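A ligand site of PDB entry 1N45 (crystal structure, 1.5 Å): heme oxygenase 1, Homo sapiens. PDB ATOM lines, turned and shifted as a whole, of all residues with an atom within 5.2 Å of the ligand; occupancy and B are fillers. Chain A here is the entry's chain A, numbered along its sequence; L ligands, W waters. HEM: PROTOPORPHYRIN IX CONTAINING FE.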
ATOM      1  N   SER A  14      11.666  25.255 -26.265  1.00  0.00           N
ATOM      2  CA  SER A  14      12.706  25.137 -25.243  1.00  0.00           C
ATOM      3  C   SER A  14      12.085  24.985 -23.845  1.00  0.00           C
ATOM      4  O   SER A  14      12.638  24.194 -23.069  1.00  0.00           O
ATOM      5  CB  SER A  14      13.615  26.363 -25.323  1.00  0.00           C
ATOM      6  OG  SER A  14      12.860  27.481 -24.855  1.00  0.00           O
ATOM      7  N   LEU A  17      10.323  21.437 -23.594  1.00  0.00           N
ATOM      8  CA  LEU A  17      11.319  20.394 -23.330  1.00  0.00           C
ATOM      9  C   LEU A  17      11.726  20.363 -21.878  1.00  0.00           C
ATOM     10  O   LEU A  17      11.799  19.309 -21.262  1.00  0.00           O
ATOM     11  CB  LEU A  17      12.551  20.582 -24.213  1.00  0.00           C
ATOM     12  CG  LEU A  17      12.373  20.187 -25.691  1.00  0.00           C
ATOM     13  CD1 LEU A  17      13.473  20.737 -26.585  1.00  0.00           C
ATOM     14  CD2 LEU A  17      12.336  18.668 -25.878  1.00  0.00           C
ATOM     15  N   LYS A  18      11.999  21.563 -21.380  1.00  0.00           N
ATOM     16  CA  LYS A  18      12.424  21.680 -19.978  1.00  0.00           C
ATOM     17  C   LYS A  18      11.348  21.115 -19.052  1.00  0.00           C
ATOM     18  O   LYS A  18      11.644  20.337 -18.148  1.00  0.00           O
ATOM     19  CB  LYS A  18      12.754  23.139 -19.663  1.00  0.00           C
ATOM     20  CG  LYS A  18      12.901  23.490 -18.192  1.00  0.00           C
ATOM     21  CD  LYS A  18      14.073  24.397 -17.896  1.00  0.00           C
ATOM     22  CE  LYS A  18      13.916  25.197 -16.609  1.00  0.00           C
ATOM     23  NZ  LYS A  18      14.963  26.252 -16.511  1.00  0.00           N
ATOM     24  N   HIS A  25      14.745  14.041 -15.504  1.00  0.00           N
ATOM     25  CA  HIS A  25      16.020  14.586 -15.006  1.00  0.00           C
ATOM     26  C   HIS A  25      16.220  14.166 -13.555  1.00  0.00           C
ATOM     27  O   HIS A  25      17.273  13.795 -13.039  1.00  0.00           O
ATOM     28  CB  HIS A  25      16.057  16.116 -15.178  1.00  0.00           C
ATOM     29  CG  HIS A  25      17.391  16.760 -14.918  1.00  0.00           C
ATOM     30  ND1 HIS A  25      17.883  16.955 -13.633  1.00  0.00           N
ATOM     31  CD2 HIS A  25      18.353  17.222 -15.736  1.00  0.00           C
ATOM     32  CE1 HIS A  25      19.073  17.514 -13.698  1.00  0.00           C
ATOM     33  NE2 HIS A  25      19.380  17.695 -14.969  1.00  0.00           N
ATOM     34  N   ALA A  28      17.379  10.717 -13.206  1.00  0.00           N
ATOM     35  CA  ALA A  28      18.819  10.644 -13.469  1.00  0.00           C
ATOM     36  C   ALA A  28      19.628  11.074 -12.242  1.00  0.00           C
ATOM     37  O   ALA A  28      20.621  10.449 -11.876  1.00  0.00           O
ATOM     38  CB  ALA A  28      19.164  11.463 -14.722  1.00  0.00           C
ATOM     39  N   GLU A  29      19.158  12.156 -11.594  1.00  0.00           N
ATOM     40  CA  GLU A  29      19.781  12.622 -10.384  1.00  0.00           C
ATOM     41  C   GLU A  29      19.673  11.559  -9.280  1.00  0.00           C
ATOM     42  O   GLU A  29      20.519  11.585  -8.371  1.00  0.00           O
ATOM     43  CB  GLU A  29      19.169  13.911  -9.807  1.00  0.00           C
ATOM     44  CG  GLU A  29      19.319  15.141 -10.683  1.00  0.00           C
ATOM     45  CD  GLU A  29      18.424  16.253 -10.180  1.00  0.00           C
ATOM     46  OE1 GLU A  29      18.700  16.745  -9.068  1.00  0.00           O
ATOM     47  OE2 GLU A  29      17.453  16.631 -10.849  1.00  0.00           O
ATOM     48  N   MET A  34      24.768   8.126 -10.066  1.00  0.00           N
ATOM     49  CA  MET A  34      24.789   9.579  -9.862  1.00  0.00           C
ATOM     50  C   MET A  34      24.590   9.963  -8.408  1.00  0.00           C
ATOM     51  O   MET A  34      25.151  10.983  -8.016  1.00  0.00           O
ATOM     52  CB  MET A  34      23.715  10.203 -10.748  1.00  0.00           C
ATOM     53  CG  MET A  34      24.069  10.035 -12.224  1.00  0.00           C
ATOM     54  SD  MET A  34      25.361  11.176 -12.693  1.00  0.00           S
ATOM     55  CE  MET A  34      26.784  10.133 -12.852  1.00  0.00           C
ATOM     56  N   GLN A  38      27.328  12.398  -6.788  1.00  0.00           N
ATOM     57  CA  GLN A  38      26.944  13.582  -6.012  1.00  0.00           C
ATOM     58  C   GLN A  38      27.391  13.509  -4.562  1.00  0.00           C
ATOM     59  O   GLN A  38      27.768  14.500  -3.925  1.00  0.00           O
ATOM     60  CB  GLN A  38      25.437  13.788  -6.097  1.00  0.00           C
ATOM     61  CG  GLN A  38      24.854  14.245  -7.416  1.00  0.00           C
ATOM     62  CD  GLN A  38      23.323  14.216  -7.395  1.00  0.00           C
ATOM     63  OE1 GLN A  38      22.654  15.186  -7.007  1.00  0.00           O
ATOM     64  NE2 GLN A  38      22.737  13.090  -7.811  1.00  0.00           N
ATOM     65  N   TYR A 114      22.708   3.450 -26.858  1.00  0.00           N
ATOM     66  CA  TYR A 114      22.608   4.899 -27.023  1.00  0.00           C
ATOM     67  C   TYR A 114      23.134   5.323 -28.411  1.00  0.00           C
ATOM     68  O   TYR A 114      22.474   6.100 -29.114  1.00  0.00           O
ATOM     69  CB  TYR A 114      23.327   5.575 -25.883  1.00  0.00           C
ATOM     70  CG  TYR A 114      23.085   7.027 -25.571  1.00  0.00           C
ATOM     71  CD1 TYR A 114      22.514   7.924 -26.460  1.00  0.00           C
ATOM     72  CD2 TYR A 114      23.479   7.539 -24.329  1.00  0.00           C
ATOM     73  CE1 TYR A 114      22.329   9.253 -26.130  1.00  0.00           C
ATOM     74  CE2 TYR A 114      23.285   8.873 -23.994  1.00  0.00           C
ATOM     75  CZ  TYR A 114      22.713   9.735 -24.895  1.00  0.00           C
ATOM     76  OH  TYR A 114      22.538  11.054 -24.536  1.00  0.00           O
ATOM     77  N   TYR A 134      19.882  18.893 -27.554  1.00  0.00           N
ATOM     78  CA  TYR A 134      19.397  19.547 -26.339  1.00  0.00           C
ATOM     79  C   TYR A 134      19.827  18.769 -25.107  1.00  0.00           C
ATOM     80  O   TYR A 134      20.447  19.366 -24.225  1.00  0.00           O
ATOM     81  CB  TYR A 134      17.863  19.617 -26.333  1.00  0.00           C
ATOM     82  CG  TYR A 134      17.174  19.903 -25.027  1.00  0.00           C
ATOM     83  CD1 TYR A 134      17.131  21.210 -24.548  1.00  0.00           C
ATOM     84  CD2 TYR A 134      16.564  18.891 -24.277  1.00  0.00           C
ATOM     85  CE1 TYR A 134      16.508  21.529 -23.360  1.00  0.00           C
ATOM     86  CE2 TYR A 134      15.949  19.196 -23.083  1.00  0.00           C
ATOM     87  CZ  TYR A 134      15.935  20.504 -22.644  1.00  0.00           C
ATOM     88  OH  TYR A 134      15.322  20.782 -21.464  1.00  0.00           O
ATOM     89  N   THR A 135      19.486  17.462 -25.072  1.00  0.00           N
ATOM     90  CA  THR A 135      19.718  16.703 -23.817  1.00  0.00           C
ATOM     91  C   THR A 135      21.195  16.677 -23.440  1.00  0.00           C
ATOM     92  O   THR A 135      21.608  16.847 -22.283  1.00  0.00           O
ATOM     93  CB  THR A 135      19.143  15.293 -24.021  1.00  0.00           C
ATOM     94  OG1 THR A 135      17.704  15.442 -24.068  1.00  0.00           O
ATOM     95  CG2 THR A 135      19.416  14.356 -22.868  1.00  0.00           C
ATOM     96  N   ARG A 136      22.077  16.453 -24.427  1.00  0.00           N
ATOM     97  CA  ARG A 136      23.526  16.357 -24.222  1.00  0.00           C
ATOM     98  C   ARG A 136      24.108  17.764 -24.068  1.00  0.00           C
ATOM     99  O   ARG A 136      24.683  18.052 -23.000  1.00  0.00           O
ATOM    100  CB  ARG A 136      24.182  15.611 -25.391  1.00  0.00           C
ATOM    101  CG  ARG A 136      24.174  14.099 -25.235  1.00  0.00           C
ATOM    102  CD  ARG A 136      25.459  13.646 -24.603  1.00  0.00           C
ATOM    103  NE  ARG A 136      25.645  14.011 -23.189  1.00  0.00           N
ATOM    104  CZ  ARG A 136      25.214  13.270 -22.219  1.00  0.00           C
ATOM    105  NH1 ARG A 136      24.505  12.131 -22.390  1.00  0.00           N
ATOM    106  NH2 ARG A 136      25.454  13.657 -20.997  1.00  0.00           N
ATOM    107  N   LEU A 138      22.873  21.002 -23.861  1.00  0.00           N
ATOM    108  CA  LEU A 138      22.397  22.030 -22.912  1.00  0.00           C
ATOM    109  C   LEU A 138      22.555  21.461 -21.512  1.00  0.00           C
ATOM    110  O   LEU A 138      22.844  22.182 -20.559  1.00  0.00           O
ATOM    111  CB  LEU A 138      20.996  22.500 -23.255  1.00  0.00           C
ATOM    112  CG  LEU A 138      20.573  23.896 -22.818  1.00  0.00           C
ATOM    113  CD1 LEU A 138      21.519  24.968 -23.355  1.00  0.00           C
ATOM    114  CD2 LEU A 138      19.127  24.181 -23.225  1.00  0.00           C
ATOM    115  N   GLY A 139      22.393  20.150 -21.373  1.00  0.00           N
ATOM    116  CA  GLY A 139      22.685  19.550 -20.088  1.00  0.00           C
ATOM    117  C   GLY A 139      24.145  19.654 -19.718  1.00  0.00           C
ATOM    118  O   GLY A 139      24.410  20.048 -18.569  1.00  0.00           O
ATOM    119  N   SER A 142      24.900  23.389 -18.957  1.00  0.00           N
ATOM    120  CA  SER A 142      24.138  23.901 -17.841  1.00  0.00           C
ATOM    121  C   SER A 142      24.565  23.269 -16.520  1.00  0.00           C
ATOM    122  O   SER A 142      24.632  23.921 -15.476  1.00  0.00           O
ATOM    123  CB  SER A 142      22.633  23.643 -17.984  1.00  0.00           C
ATOM    124  OG  SER A 142      21.908  24.838 -17.866  1.00  0.00           O
ATOM    125  N   GLY A 143      24.839  21.975 -16.611  1.00  0.00           N
ATOM    126  CA  GLY A 143      25.249  21.213 -15.449  1.00  0.00           C
ATOM    127  C   GLY A 143      26.742  21.054 -15.283  1.00  0.00           C
ATOM    128  O   GLY A 143      27.172  20.595 -14.235  1.00  0.00           O
ATOM    129  N   VAL A 146      28.555  22.233 -11.850  1.00  0.00           N
ATOM    130  CA  VAL A 146      28.519  21.450 -10.602  1.00  0.00           C
ATOM    131  C   VAL A 146      29.173  20.091 -10.848  1.00  0.00           C
ATOM    132  O   VAL A 146      29.828  19.524  -9.970  1.00  0.00           O
ATOM    133  CB  VAL A 146      27.116  21.266 -10.002  1.00  0.00           C
ATOM    134  CG1 VAL A 146      26.171  22.413 -10.349  1.00  0.00           C
ATOM    135  CG2 VAL A 146      26.491  19.945 -10.462  1.00  0.00           C
ATOM    136  N   LEU A 147      29.021  19.576 -12.057  1.00  0.00           N
ATOM    137  CA  LEU A 147      29.450  18.209 -12.404  1.00  0.00           C
ATOM    138  C   LEU A 147      30.965  18.115 -12.353  1.00  0.00           C
ATOM    139  O   LEU A 147      31.554  17.149 -11.883  1.00  0.00           O
ATOM    140  CB  LEU A 147      28.889  17.790 -13.776  1.00  0.00           C
ATOM    141  CG  LEU A 147      27.366  17.826 -13.999  1.00  0.00           C
ATOM    142  CD1 LEU A 147      26.991  17.768 -15.485  1.00  0.00           C
ATOM    143  CD2 LEU A 147      26.634  16.694 -13.288  1.00  0.00           C
ATOM    144  N   LYS A 179      23.158  29.751 -23.814  1.00  0.00           N
ATOM    145  CA  LYS A 179      21.921  28.997 -23.614  1.00  0.00           C
ATOM    146  C   LYS A 179      20.707  29.762 -24.111  1.00  0.00           C
ATOM    147  O   LYS A 179      19.715  29.272 -24.632  1.00  0.00           O
ATOM    148  CB  LYS A 179      21.769  28.658 -22.128  1.00  0.00           C
ATOM    149  CG  LYS A 179      22.873  27.774 -21.584  1.00  0.00           C
ATOM    150  CD  LYS A 179      22.867  27.729 -20.041  1.00  0.00           C
ATOM    151  CE  LYS A 179      21.466  27.380 -19.577  1.00  0.00           C
ATOM    152  NZ  LYS A 179      21.020  26.057 -20.131  1.00  0.00           N
ATOM    153  N   ARG A 183      18.414  28.420 -27.006  1.00  0.00           N
ATOM    154  CA  ARG A 183      16.968  28.215 -26.845  1.00  0.00           C
ATOM    155  C   ARG A 183      16.177  28.971 -27.913  1.00  0.00           C
ATOM    156  O   ARG A 183      15.167  28.519 -28.457  1.00  0.00           O
ATOM    157  CB  ARG A 183      16.598  28.604 -25.418  1.00  0.00           C
ATOM    158  CG  ARG A 183      17.212  27.653 -24.383  1.00  0.00           C
ATOM    159  CD  ARG A 183      16.635  28.137 -23.064  1.00  0.00           C
ATOM    160  NE  ARG A 183      17.048  27.371 -21.915  1.00  0.00           N
ATOM    161  CZ  ARG A 183      17.819  27.745 -20.911  1.00  0.00           C
ATOM    162  NH1 ARG A 183      18.360  28.962 -20.788  1.00  0.00           N
ATOM    163  NH2 ARG A 183      18.057  26.851 -19.943  1.00  0.00           N
ATOM    164  N   PHE A 207      17.111  10.826 -22.056  1.00  0.00           N
ATOM    165  CA  PHE A 207      17.374  10.710 -20.628  1.00  0.00           C
ATOM    166  C   PHE A 207      17.357   9.248 -20.210  1.00  0.00           C
ATOM    167  O   PHE A 207      18.212   8.786 -19.455  1.00  0.00           O
ATOM    168  CB  PHE A 207      16.349  11.471 -19.799  1.00  0.00           C
ATOM    169  CG  PHE A 207      16.670  12.942 -19.595  1.00  0.00           C
ATOM    170  CD1 PHE A 207      16.249  13.915 -20.487  1.00  0.00           C
ATOM    171  CD2 PHE A 207      17.400  13.368 -18.495  1.00  0.00           C
ATOM    172  CE1 PHE A 207      16.564  15.234 -20.274  1.00  0.00           C
ATOM    173  CE2 PHE A 207      17.698  14.706 -18.284  1.00  0.00           C
ATOM    174  CZ  PHE A 207      17.279  15.652 -19.189  1.00  0.00           C
ATOM    175  N   ASN A 210      20.519   7.476 -20.986  1.00  0.00           N
ATOM    176  CA  ASN A 210      21.552   7.822 -20.021  1.00  0.00           C
ATOM    177  C   ASN A 210      21.380   7.050 -18.704  1.00  0.00           C
ATOM    178  O   ASN A 210      22.331   6.501 -18.137  1.00  0.00           O
ATOM    179  CB  ASN A 210      21.507   9.328 -19.763  1.00  0.00           C
ATOM    180  CG  ASN A 210      22.253  10.134 -20.799  1.00  0.00           C
ATOM    181  OD1 ASN A 210      23.459  10.372 -20.760  1.00  0.00           O
ATOM    182  ND2 ASN A 210      21.501  10.587 -21.787  1.00  0.00           N
ATOM    183  N   PHE A 214      23.827   4.427 -16.775  1.00  0.00           N
ATOM    184  CA  PHE A 214      24.294   4.616 -15.417  1.00  0.00           C
ATOM    185  C   PHE A 214      24.073   3.323 -14.617  1.00  0.00           C
ATOM    186  O   PHE A 214      24.944   2.958 -13.844  1.00  0.00           O
ATOM    187  CB  PHE A 214      23.600   5.751 -14.694  1.00  0.00           C
ATOM    188  CG  PHE A 214      23.740   7.160 -15.245  1.00  0.00           C
ATOM    189  CD1 PHE A 214      24.796   7.525 -16.051  1.00  0.00           C
ATOM    190  CD2 PHE A 214      22.768   8.109 -14.924  1.00  0.00           C
ATOM    191  CE1 PHE A 214      24.894   8.830 -16.547  1.00  0.00           C
ATOM    192  CE2 PHE A 214      22.875   9.391 -15.403  1.00  0.00           C
ATOM    193  CZ  PHE A 214      23.935   9.765 -16.212  1.00  0.00           C
HETATM  194  CHA HEM L   1      20.179  21.228 -16.420  1.00  0.00           C
HETATM  195  CHB HEM L   1      22.716  19.165 -12.908  1.00  0.00           C
HETATM  196  CHC HEM L   1      21.957  14.855 -14.793  1.00  0.00           C
HETATM  197  CHD HEM L   1      20.397  17.067 -18.833  1.00  0.00           C
HETATM  198  C1A HEM L   1      20.654  21.007 -15.121  1.00  0.00           C
HETATM  199  C2A HEM L   1      21.254  22.087 -14.379  1.00  0.00           C
HETATM  200  C3A HEM L   1      22.149  21.536 -13.535  1.00  0.00           C
HETATM  201  C4A HEM L   1      22.089  20.115 -13.727  1.00  0.00           C
HETATM  202  CMA HEM L   1      22.905  22.160 -12.349  1.00  0.00           C
HETATM  203  CAA HEM L   1      20.750  23.514 -14.321  1.00  0.00           C
HETATM  204  CBA HEM L   1      19.277  23.782 -14.562  1.00  0.00           C
HETATM  205  CGA HEM L   1      18.992  24.923 -15.526  1.00  0.00           C
HETATM  206  O1A HEM L   1      18.660  26.023 -15.015  1.00  0.00           O
HETATM  207  O2A HEM L   1      19.050  24.784 -16.782  1.00  0.00           O
HETATM  208  C1B HEM L   1      22.302  17.820 -12.890  1.00  0.00           C
HETATM  209  C2B HEM L   1      22.871  16.904 -11.943  1.00  0.00           C
HETATM  210  C3B HEM L   1      22.742  15.679 -12.503  1.00  0.00           C
HETATM  211  C4B HEM L   1      22.216  15.859 -13.844  1.00  0.00           C
HETATM  212  CMB HEM L   1      23.440  17.255 -10.556  1.00  0.00           C
HETATM  213  CAB HEM L   1      22.963  14.448 -11.923  1.00  0.00           C
HETATM  214  CBB HEM L   1      23.441  13.975 -10.740  1.00  0.00           C
HETATM  215  C1C HEM L   1      21.693  15.122 -16.156  1.00  0.00           C
HETATM  216  C2C HEM L   1      21.594  14.107 -17.176  1.00  0.00           C
HETATM  217  C3C HEM L   1      21.145  14.729 -18.287  1.00  0.00           C
HETATM  218  C4C HEM L   1      20.957  16.117 -17.952  1.00  0.00           C
HETATM  219  CMC HEM L   1      21.950  12.640 -16.963  1.00  0.00           C
HETATM  220  CAC HEM L   1      21.065  14.237 -19.595  1.00  0.00           C
HETATM  221  CBC HEM L   1      21.928  13.357 -20.184  1.00  0.00           C
HETATM  222  C1D HEM L   1      20.007  18.347 -18.444  1.00  0.00           C
HETATM  223  C2D HEM L   1      19.378  19.307 -19.319  1.00  0.00           C
HETATM  224  C3D HEM L   1      19.327  20.480 -18.657  1.00  0.00           C
HETATM  225  C4D HEM L   1      19.944  20.246 -17.371  1.00  0.00           C
HETATM  226  CMD HEM L   1      19.010  18.971 -20.777  1.00  0.00           C
HETATM  227  CAD HEM L   1      18.873  21.833 -19.176  1.00  0.00           C
HETATM  228  CBD HEM L   1      17.413  22.149 -18.925  1.00  0.00           C
HETATM  229  CGD HEM L   1      16.851  23.281 -19.751  1.00  0.00           C
HETATM  230  O1D HEM L   1      15.955  23.039 -20.572  1.00  0.00           O
HETATM  231  O2D HEM L   1      17.292  24.440 -19.584  1.00  0.00           O
HETATM  232  NA  HEM L   1      21.181  19.785 -14.718  1.00  0.00           N
HETATM  233  NB  HEM L   1      21.936  17.194 -14.084  1.00  0.00           N
HETATM  234  NC  HEM L   1      21.225  16.335 -16.627  1.00  0.00           N
HETATM  235  ND  HEM L   1      20.467  18.954 -17.294  1.00  0.00           N
HETATM  236 FE   HEM L   1      21.187  18.077 -15.704  1.00  0.00          FE
HETATM  237  O   HOH W   1      23.024  18.513 -16.487  1.00  0.00           O
HETATM  238  O   HOH W   2      15.219  25.101 -21.971  1.00  0.00           O
HETATM  239  O   HOH W   3      20.123  27.324 -17.129  1.00  0.00           O
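The side-chain carboxylate (OE2) of Glu 29 lies within hydrogen-bond range of a ring nitrogen (ND1) of His 25 (2.8 Å).
The side-chain hydroxyl of Tyr 134 lies close to the backbone NH of Lys 18, at 3.4 Å.
OG of Ser 142 is in hydrogen-bond range of NZ of Lys 179 (2.7 Å).
NE2 of Gln 38 sits at hydrogen-bond distance from O of Met 34 (3.2 Å).
The backbone carbonyl oxygen (O) of Glu 29 is in hydrogen-bond range of the side-chain amide nitrogen (NE2) of Gln 38 (2.7 Å).
The guanidinium group of Arg 136 is in hydrogen-bond range of the side-chain amide oxygen of Asn 210, 2.6 Å away.
ND2 of Asn 210 lies within hydrogen-bond range of OH of Tyr 114 (3.0 Å).
NH1 of Arg 136 lies within hydrogen-bond range of OH of Tyr 114 (3.1 Å).
A ring nitrogen (NE2) of His 25 binds an iron atom (FE) of the ligand.
The side-chain hydroxyl of Tyr 134 lies within hydrogen-bond range of an oxygen (O1D) of the ligand.
O2D of the ligand lies within salt-bridge range of NH2 of Arg 183 (2.6 Å).
O2A of the ligand is in hydrogen-bond range of OG of Ser 142, at 3.1 Å.
The side-chain amino group (NZ) of Lys 18 lies within salt-bridge range of an oxygen (O1A) of the ligand, 3.99 Å away.
Water W2 lies within hydrogen-bond range of O1D of the ligand (2.6 Å), NE of Arg 183 (2.9 Å) and O of Ser 14 (2.9 Å).
Water W3 lies within hydrogen-bond range of an oxygen (O2A) of the ligand, the side-chain hydroxyl of Ser 142 and the side-chain amino group of Lys 179.
CB of Ala 28 touches CMC of the ligand (3.8 Å).
CG of Glu 29 touches CAB of the ligand, 3.9 Å away.
Met 34 touches the ligand.
Gln 38 touches the ligand.
Thr 135 touches the ligand (O to CHD, 3.7 Å).
NH1 of Arg 136 touches CBC of the ligand (3.6 Å).
CA of Gly 139 touches C1D of the ligand (3.4 Å).
Gly 143 touches the ligand.
CG1 of Val 146 touches CMA of the ligand, 3.8 Å away.
Phe 207 touches the ligand (CZ to CHD, 3.4 Å).
Asn 210 touches the ligand (ND2 to CBC, 3.2 Å).
CZ of Phe 214 touches CMC of the ligand, 3.6 Å away.
Hydrophobic or aromatic side chains that line the ligand: His 25, Ala 28, Met 34, Tyr 134, Val 146, Phe 207 and Phe 214.
17 residues have an atom within 4 Å of the ligand: Lys 18, His 25, Ala 28, Glu 29, Met 34, Gln 38, Tyr 134, Thr 135, Arg 136, Gly 139, Ser 142, Gly 143, Val 146, Arg 183, Phe 207, Asn 210 and Phe 214.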
